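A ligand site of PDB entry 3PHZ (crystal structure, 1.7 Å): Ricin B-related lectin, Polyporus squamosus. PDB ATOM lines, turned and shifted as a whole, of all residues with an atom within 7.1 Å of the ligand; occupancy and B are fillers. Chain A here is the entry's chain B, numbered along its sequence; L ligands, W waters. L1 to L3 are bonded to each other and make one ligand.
N of Ser 32 sits close to O1 of LG3 L3. O1 of LG3 L3 lies within hydrogen-bond range of OG of Ser 32 (2.5 Å). OD2 of Asp 72 sits at hydrogen-bond distance from O2 of LG2 L2, 2.7 Å away. An oxygen (O2) of LG2 L2 is in hydrogen-bond range of the side-chain amide nitrogen (ND2) of Asn 94, at 3.0 Å. N1 of LG3 L3 lies within hydrogen-bond range of O of Asn 30 (3.1 Å). N of Gly 75 sits at hydrogen-bond distance from O3 of LG2 L2, 3.2 Å away. NE2 of His 76 is in hydrogen-bond range of O1 of LG2 L2 (3.2 Å).
Water W1 lies within hydrogen-bond range of O2 of LG3 L3 (2.5 Å) and OH of Tyr 87 (2.9 Å). Water W2 lies within hydrogen-bond range of the side-chain hydroxyl (OG1) of Thr 90 (2.6 Å), the side-chain amide oxygen (OD1) of Asn 94 (2.6 Å) and an oxygen (O2) of LG2 L2 (2.7 Å).
The side-chain amide nitrogen (ND2) of Asn 94 lies within hydrogen-bond range of the side-chain carboxylate (OD1) of Asp 72 (2.9 Å). The backbone carbonyl oxygen (O) of Ile 85 is in hydrogen-bond range of the backbone NH (N) of Asp 72 (2.9 Å). OD2 of Asp 72 lies within hydrogen-bond range of NE2 of Gln 95, 2.9 Å away. OD1 of Asn 94 sits close to ND1 of His 76, 3.4 Å away. O of Leu 73 lies within hydrogen-bond range of ND2 of Asn 94, 2.8 Å away. N of Ala 74 lies within hydrogen-bond range of O of Ala 83 (3.1 Å).
NZ of Lys 31 touches C11 of LG3 L3, 3.5 Å away. CA of Ala 74 touches O3 of LG2 L2 (3.4 Å). CD1 of Ile 85 touches O3 of LG2 L2, 3.7 Å away. Tyr 87 touches the ligand. Hydrophobic or aromatic side chains within 4 Å of the ligand: Ile 85 and Tyr 87. Within 4 Å of the ligand: Asn 30, Lys 31, Ser 32, Asp 72, Ala 74, Gly 75, His 76, Ile 85, Tyr 87 and Asn 94.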
ATOM      1  N   ASN A  30     -26.854  10.078 -10.142  1.00  0.00           N
ATOM      2  CA  ASN A  30     -25.557  10.725 -10.296  1.00  0.00           C
ATOM      3  C   ASN A  30     -25.688  12.227 -10.685  1.00  0.00           C
ATOM      4  O   ASN A  30     -26.818  12.757 -10.872  1.00  0.00           O
ATOM      5  CB  ASN A  30     -24.650   9.930 -11.278  1.00  0.00           C
ATOM      6  CG  ASN A  30     -23.155   9.922 -10.846  1.00  0.00           C
ATOM      7  OD1 ASN A  30     -22.838   9.965  -9.650  1.00  0.00           O
ATOM      8  ND2 ASN A  30     -22.234   9.882 -11.831  1.00  0.00           N
ATOM      9  N   LYS A  31     -24.536  12.899 -10.764  1.00  0.00           N
ATOM     10  CA  LYS A  31     -24.435  14.326 -11.037  1.00  0.00           C
ATOM     11  C   LYS A  31     -23.528  14.626 -12.253  1.00  0.00           C
ATOM     12  O   LYS A  31     -22.661  13.814 -12.643  1.00  0.00           O
ATOM     13  CB  LYS A  31     -23.885  15.067  -9.808  1.00  0.00           C
ATOM     14  CG  LYS A  31     -24.249  14.519  -8.432  1.00  0.00           C
ATOM     15  CD  LYS A  31     -23.605  15.361  -7.328  1.00  0.00           C
ATOM     16  CE  LYS A  31     -23.946  14.842  -5.922  1.00  0.00           C
ATOM     17  NZ  LYS A  31     -25.400  14.959  -5.586  1.00  0.00           N
ATOM     18  N   SER A  32     -23.752  15.803 -12.838  1.00  0.00           N
ATOM     19  CA  SER A  32     -22.792  16.457 -13.729  1.00  0.00           C
ATOM     20  C   SER A  32     -21.520  16.911 -12.952  1.00  0.00           C
ATOM     21  O   SER A  32     -21.573  17.183 -11.736  1.00  0.00           O
ATOM     22  CB  SER A  32     -23.443  17.687 -14.382  1.00  0.00           C
ATOM     23  OG  SER A  32     -24.565  17.315 -15.175  1.00  0.00           O
ATOM     24  N   PRO A  33     -20.378  17.027 -13.659  1.00  0.00           N
ATOM     25  CA  PRO A  33     -19.208  17.572 -12.967  1.00  0.00           C
ATOM     26  C   PRO A  33     -19.392  19.041 -12.511  1.00  0.00           C
ATOM     27  O   PRO A  33     -19.914  19.899 -13.230  1.00  0.00           O
ATOM     28  CB  PRO A  33     -18.063  17.383 -13.994  1.00  0.00           C
ATOM     29  CG  PRO A  33     -18.711  17.119 -15.310  1.00  0.00           C
ATOM     30  CD  PRO A  33     -20.066  16.544 -15.025  1.00  0.00           C
ATOM     31  N   ASP A  34     -18.929  19.354 -11.300  1.00  0.00           N
ATOM     32  CA  ASP A  34     -19.000  20.743 -10.835  1.00  0.00           C
ATOM     33  C   ASP A  34     -17.841  21.575 -11.384  1.00  0.00           C
ATOM     34  O   ASP A  34     -16.778  21.023 -11.633  1.00  0.00           O
ATOM     35  CB  ASP A  34     -18.855  20.727  -9.311  1.00  0.00           C
ATOM     36  CG  ASP A  34     -20.045  20.010  -8.685  1.00  0.00           C
ATOM     37  OD1 ASP A  34     -21.149  20.564  -8.901  1.00  0.00           O
ATOM     38  OD2 ASP A  34     -19.836  18.895  -8.119  1.00  0.00           O
ATOM     39  N   ASP A  72     -22.682  26.444 -16.272  1.00  0.00           N
ATOM     40  CA  ASP A  72     -24.152  26.265 -16.279  1.00  0.00           C
ATOM     41  C   ASP A  72     -24.590  26.402 -14.799  1.00  0.00           C
ATOM     42  O   ASP A  72     -24.057  25.691 -13.906  1.00  0.00           O
ATOM     43  CB  ASP A  72     -24.445  24.891 -16.850  1.00  0.00           C
ATOM     44  CG  ASP A  72     -25.923  24.507 -16.796  1.00  0.00           C
ATOM     45  OD1 ASP A  72     -26.517  24.720 -15.723  1.00  0.00           O
ATOM     46  OD2 ASP A  72     -26.457  23.912 -17.785  1.00  0.00           O
ATOM     47  N   LEU A  73     -25.476  27.380 -14.556  1.00  0.00           N
ATOM     48  CA  LEU A  73     -26.121  27.515 -13.195  1.00  0.00           C
ATOM     49  C   LEU A  73     -27.207  26.472 -13.084  1.00  0.00           C
ATOM     50  O   LEU A  73     -28.254  26.554 -13.804  1.00  0.00           O
ATOM     51  CB  LEU A  73     -26.648  28.907 -13.016  1.00  0.00           C
ATOM     52  CG  LEU A  73     -27.255  29.233 -11.621  1.00  0.00           C
ATOM     53  CD1 LEU A  73     -26.261  28.970 -10.497  1.00  0.00           C
ATOM     54  CD2 LEU A  73     -27.562  30.680 -11.636  1.00  0.00           C
ATOM     55  N   ALA A  74     -26.961  25.483 -12.233  1.00  0.00           N
ATOM     56  CA  ALA A  74     -27.670  24.221 -12.231  1.00  0.00           C
ATOM     57  C   ALA A  74     -29.181  24.452 -12.000  1.00  0.00           C
ATOM     58  O   ALA A  74     -29.612  24.422 -10.861  1.00  0.00           O
ATOM     59  CB  ALA A  74     -27.093  23.343 -11.167  1.00  0.00           C
ATOM     60  N   GLY A  75     -29.958  24.758 -13.075  1.00  0.00           N
ATOM     61  CA  GLY A  75     -31.420  24.726 -13.010  1.00  0.00           C
ATOM     62  C   GLY A  75     -32.049  26.077 -13.057  1.00  0.00           C
ATOM     63  O   GLY A  75     -33.219  26.275 -12.618  1.00  0.00           O
ATOM     64  N   HIS A  76     -31.331  27.035 -13.600  1.00  0.00           N
ATOM     65  CA  HIS A  76     -31.839  28.371 -13.615  1.00  0.00           C
ATOM     66  C   HIS A  76     -32.158  28.665 -12.122  1.00  0.00           C
ATOM     67  O   HIS A  76     -32.630  29.777 -11.859  1.00  0.00           O
ATOM     68  CB  HIS A  76     -33.087  28.483 -14.560  1.00  0.00           C
ATOM     69  CG  HIS A  76     -33.042  27.539 -15.747  1.00  0.00           C
ATOM     70  ND1 HIS A  76     -32.684  27.946 -17.013  1.00  0.00           N
ATOM     71  CD2 HIS A  76     -33.241  26.192 -15.824  1.00  0.00           C
ATOM     72  CE1 HIS A  76     -32.721  26.903 -17.836  1.00  0.00           C
ATOM     73  NE2 HIS A  76     -33.027  25.822 -17.138  1.00  0.00           N
ATOM     74  N   THR A  82     -26.506  27.317  -5.126  1.00  0.00           N
ATOM     75  CA  THR A  82     -26.799  26.443  -6.282  1.00  0.00           C
ATOM     76  C   THR A  82     -25.484  26.096  -7.004  1.00  0.00           C
ATOM     77  O   THR A  82     -24.725  27.020  -7.249  1.00  0.00           O
ATOM     78  CB  THR A  82     -27.751  27.138  -7.221  1.00  0.00           C
ATOM     79  OG1 THR A  82     -29.065  27.103  -6.608  1.00  0.00           O
ATOM     80  CG2 THR A  82     -27.857  26.394  -8.543  1.00  0.00           C
ATOM     81  N   ALA A  83     -25.240  24.802  -7.271  1.00  0.00           N
ATOM     82  CA  ALA A  83     -24.047  24.314  -8.006  1.00  0.00           C
ATOM     83  C   ALA A  83     -23.845  25.085  -9.324  1.00  0.00           C
ATOM     84  O   ALA A  83     -24.789  25.427 -10.054  1.00  0.00           O
ATOM     85  CB  ALA A  83     -24.066  22.864  -8.195  1.00  0.00           C
ATOM     86  N   ILE A  84     -22.589  25.493  -9.546  1.00  0.00           N
ATOM     87  CA  ILE A  84     -22.169  25.864 -10.902  1.00  0.00           C
ATOM     88  C   ILE A  84     -21.488  24.593 -11.480  1.00  0.00           C
ATOM     89  O   ILE A  84     -20.603  23.974 -10.863  1.00  0.00           O
ATOM     90  CB  ILE A  84     -21.311  27.172 -10.909  1.00  0.00           C
ATOM     91  CG1 ILE A  84     -22.243  28.329 -10.448  1.00  0.00           C
ATOM     92  CG2 ILE A  84     -20.742  27.377 -12.350  1.00  0.00           C
ATOM     93  CD1 ILE A  84     -21.686  29.684 -10.543  1.00  0.00           C
ATOM     94  N   ILE A  85     -21.978  24.125 -12.656  1.00  0.00           N
ATOM     95  CA  ILE A  85     -21.617  22.835 -13.226  1.00  0.00           C
ATOM     96  C   ILE A  85     -21.133  23.069 -14.682  1.00  0.00           C
ATOM     97  O   ILE A  85     -21.300  24.169 -15.222  1.00  0.00           O
ATOM     98  CB  ILE A  85     -22.768  21.793 -13.266  1.00  0.00           C
ATOM     99  CG1 ILE A  85     -23.955  22.348 -14.076  1.00  0.00           C
ATOM    100  CG2 ILE A  85     -23.156  21.362 -11.785  1.00  0.00           C
ATOM    101  CD1 ILE A  85     -25.184  21.340 -14.044  1.00  0.00           C
ATOM    102  N   GLY A  86     -20.591  22.003 -15.245  1.00  0.00           N
ATOM    103  CA  GLY A  86     -20.165  21.926 -16.644  1.00  0.00           C
ATOM    104  C   GLY A  86     -21.231  21.095 -17.265  1.00  0.00           C
ATOM    105  O   GLY A  86     -21.392  19.925 -16.926  1.00  0.00           O
ATOM    106  N   TYR A  87     -21.926  21.665 -18.248  1.00  0.00           N
ATOM    107  CA  TYR A  87     -23.057  20.925 -18.841  1.00  0.00           C
ATOM    108  C   TYR A  87     -23.064  21.013 -20.354  1.00  0.00           C
ATOM    109  O   TYR A  87     -22.594  21.974 -20.924  1.00  0.00           O
ATOM    110  CB  TYR A  87     -24.360  21.601 -18.354  1.00  0.00           C
ATOM    111  CG  TYR A  87     -25.612  20.696 -18.408  1.00  0.00           C
ATOM    112  CD1 TYR A  87     -25.759  19.571 -17.568  1.00  0.00           C
ATOM    113  CD2 TYR A  87     -26.670  20.998 -19.295  1.00  0.00           C
ATOM    114  CE1 TYR A  87     -26.888  18.754 -17.652  1.00  0.00           C
ATOM    115  CE2 TYR A  87     -27.825  20.163 -19.378  1.00  0.00           C
ATOM    116  CZ  TYR A  87     -27.932  19.059 -18.536  1.00  0.00           C
ATOM    117  OH  TYR A  87     -29.068  18.252 -18.603  1.00  0.00           O
ATOM    118  N   ARG A  88     -23.699  20.044 -21.015  1.00  0.00           N
ATOM    119  CA  ARG A  88     -23.832  20.144 -22.487  1.00  0.00           C
ATOM    120  C   ARG A  88     -24.475  21.481 -22.868  1.00  0.00           C
ATOM    121  O   ARG A  88     -25.262  22.048 -22.094  1.00  0.00           O
ATOM    122  CB  ARG A  88     -24.625  18.993 -23.024  1.00  0.00           C
ATOM    123  CG  ARG A  88     -26.091  18.955 -22.458  1.00  0.00           C
ATOM    124  CD  ARG A  88     -26.934  17.802 -23.114  1.00  0.00           C
ATOM    125  NE  ARG A  88     -28.360  17.919 -22.741  1.00  0.00           N
ATOM    126  CZ  ARG A  88     -29.282  18.764 -23.239  1.00  0.00           C
ATOM    127  NH1 ARG A  88     -29.023  19.698 -24.175  1.00  0.00           N
ATOM    128  NH2 ARG A  88     -30.504  18.707 -22.761  1.00  0.00           N
ATOM    129  N   THR A  90     -27.127  24.036 -24.130  1.00  0.00           N
ATOM    130  CA  THR A  90     -28.605  23.868 -24.172  1.00  0.00           C
ATOM    131  C   THR A  90     -29.293  24.996 -24.914  1.00  0.00           C
ATOM    132  O   THR A  90     -30.503  24.865 -25.208  1.00  0.00           O
ATOM    133  CB  THR A  90     -29.128  23.939 -22.710  1.00  0.00           C
ATOM    134  OG1 THR A  90     -28.742  25.186 -22.160  1.00  0.00           O
ATOM    135  CG2 THR A  90     -28.702  22.679 -21.942  1.00  0.00           C
ATOM    136  N   GLY A  92     -29.799  27.569 -23.370  1.00  0.00           N
ATOM    137  CA  GLY A  92     -30.425  28.149 -22.141  1.00  0.00           C
ATOM    138  C   GLY A  92     -29.778  29.408 -21.568  1.00  0.00           C
ATOM    139  O   GLY A  92     -28.579  29.726 -21.756  1.00  0.00           O
ATOM    140  N   ASN A  94     -29.406  29.980 -18.426  1.00  0.00           N
ATOM    141  CA  ASN A  94     -28.506  29.535 -17.277  1.00  0.00           C
ATOM    142  C   ASN A  94     -27.070  29.145 -17.826  1.00  0.00           C
ATOM    143  O   ASN A  94     -26.276  28.620 -17.055  1.00  0.00           O
ATOM    144  CB  ASN A  94     -29.089  28.428 -16.413  1.00  0.00           C
ATOM    145  CG  ASN A  94     -29.240  27.167 -17.109  1.00  0.00           C
ATOM    146  OD1 ASN A  94     -29.615  27.175 -18.298  1.00  0.00           O
ATOM    147  ND2 ASN A  94     -28.988  26.041 -16.445  1.00  0.00           N
ATOM    148  N   GLN A  95     -26.791  29.399 -19.116  1.00  0.00           N
ATOM    149  CA  GLN A  95     -25.410  29.146 -19.684  1.00  0.00           C
ATOM    150  C   GLN A  95     -24.849  30.441 -20.226  1.00  0.00           C
ATOM    151  O   GLN A  95     -23.823  30.514 -20.966  1.00  0.00           O
ATOM    152  CB  GLN A  95     -25.424  27.983 -20.722  1.00  0.00           C
ATOM    153  CG  GLN A  95     -25.865  26.643 -20.116  1.00  0.00           C
ATOM    154  CD  GLN A  95     -25.568  25.536 -21.050  1.00  0.00           C
ATOM    155  OE1 GLN A  95     -25.350  25.781 -22.272  1.00  0.00           O
ATOM    156  NE2 GLN A  95     -25.546  24.351 -20.541  1.00  0.00           N
HETATM  157  C1  LIG L   1     -35.655  20.029 -13.300  1.00  0.00           C
HETATM  158  C2  LIG L   1     -34.515  19.019 -13.457  1.00  0.00           C
HETATM  159  C3  LIG L   1     -33.252  19.651 -14.064  1.00  0.00           C
HETATM  160  C4  LIG L   1     -33.555  20.664 -15.201  1.00  0.00           C
HETATM  161  C5  LIG L   1     -34.854  21.472 -15.007  1.00  0.00           C
HETATM  162  C6  LIG L   1     -35.205  22.058 -16.372  1.00  0.00           C
HETATM  163  C7  LIG L   1     -34.365  16.981 -12.019  1.00  0.00           C
HETATM  164  C8  LIG L   1     -33.999  16.434 -10.660  1.00  0.00           C
HETATM  165  N1  LIG L   1     -34.224  18.320 -12.197  1.00  0.00           N
HETATM  166  O1  LIG L   1     -36.725  19.237 -12.865  1.00  0.00           O
HETATM  167  O2  LIG L   1     -32.506  18.541 -14.542  1.00  0.00           O
HETATM  168  O3  LIG L   1     -32.633  21.723 -15.327  1.00  0.00           O
HETATM  169  O4  LIG L   1     -35.954  20.702 -14.535  1.00  0.00           O
HETATM  170  O5  LIG L   1     -35.621  20.976 -17.148  1.00  0.00           O
HETATM  171  O6  LIG L   1     -34.766  16.206 -12.906  1.00  0.00           O
HETATM  172  C1  LG2 L   2     -31.422  21.374 -15.992  1.00  0.00           C
HETATM  173  C2  LG2 L   2     -30.895  22.589 -16.734  1.00  0.00           C
HETATM  174  C3  LG2 L   2     -29.480  22.266 -17.257  1.00  0.00           C
HETATM  175  C4  LG2 L   2     -28.576  21.775 -16.115  1.00  0.00           C
HETATM  176  C5  LG2 L   2     -29.274  20.542 -15.530  1.00  0.00           C
HETATM  177  C6  LG2 L   2     -28.616  19.870 -14.350  1.00  0.00           C
HETATM  178  O1  LG2 L   2     -31.630  22.989 -17.875  1.00  0.00           O
HETATM  179  O2  LG2 L   2     -29.078  23.432 -17.883  1.00  0.00           O
HETATM  180  O3  LG2 L   2     -28.440  22.795 -15.164  1.00  0.00           O
HETATM  181  O4  LG2 L   2     -30.508  20.937 -15.015  1.00  0.00           O
HETATM  182  O5  LG2 L   2     -29.257  18.601 -14.205  1.00  0.00           O
HETATM  183  C1  LG3 L   3     -27.742  16.741 -14.169  1.00  0.00           C
HETATM  184  C2  LG3 L   3     -29.012  17.290 -13.503  1.00  0.00           C
HETATM  185  C3  LG3 L   3     -30.019  16.194 -13.140  1.00  0.00           C
HETATM  186  C4  LG3 L   3     -29.621  15.390 -11.882  1.00  0.00           C
HETATM  187  C5  LG3 L   3     -28.929  16.200 -10.739  1.00  0.00           C
HETATM  188  C6  LG3 L   3     -27.930  17.202 -11.420  1.00  0.00           C
HETATM  189  C7  LG3 L   3     -27.035  18.295 -10.769  1.00  0.00           C
HETATM  190  C8  LG3 L   3     -27.151  18.405  -9.266  1.00  0.00           C
HETATM  191  C9  LG3 L   3     -26.074  19.395  -8.763  1.00  0.00           C
HETATM  192  C10 LG3 L   3     -28.723  15.133  -8.487  1.00  0.00           C
HETATM  193  C11 LG3 L   3     -28.053  14.068  -7.618  1.00  0.00           C
HETATM  194  N1  LG3 L   3     -28.363  15.222  -9.779  1.00  0.00           N
HETATM  195  O1  LG3 L   3     -26.592  17.160 -13.804  1.00  0.00           O
HETATM  196  O2  LG3 L   3     -27.848  15.869 -15.075  1.00  0.00           O
HETATM  197  O3  LG3 L   3     -30.823  14.774 -11.411  1.00  0.00           O
HETATM  198  O4  LG3 L   3     -28.722  18.008 -12.289  1.00  0.00           O
HETATM  199  O5  LG3 L   3     -25.646  18.242 -11.222  1.00  0.00           O
HETATM  200  O6  LG3 L   3     -28.494  18.866  -9.097  1.00  0.00           O
HETATM  201  O7  LG3 L   3     -24.844  18.647  -8.662  1.00  0.00           O
HETATM  202  O8  LG3 L   3     -29.561  15.896  -7.992  1.00  0.00           O
HETATM  203  O   HOH W   1     -29.625  16.051 -16.787  1.00  0.00           O
HETATM  204  O   HOH W   2     -30.031  25.081 -19.864  1.00  0.00           O
HETATM  205  O   HOH W   3     -31.710  20.725 -20.034  1.00  0.00           O
HETATM  206  O   HOH W   4     -33.793  20.276 -18.578  1.00  0.00           O
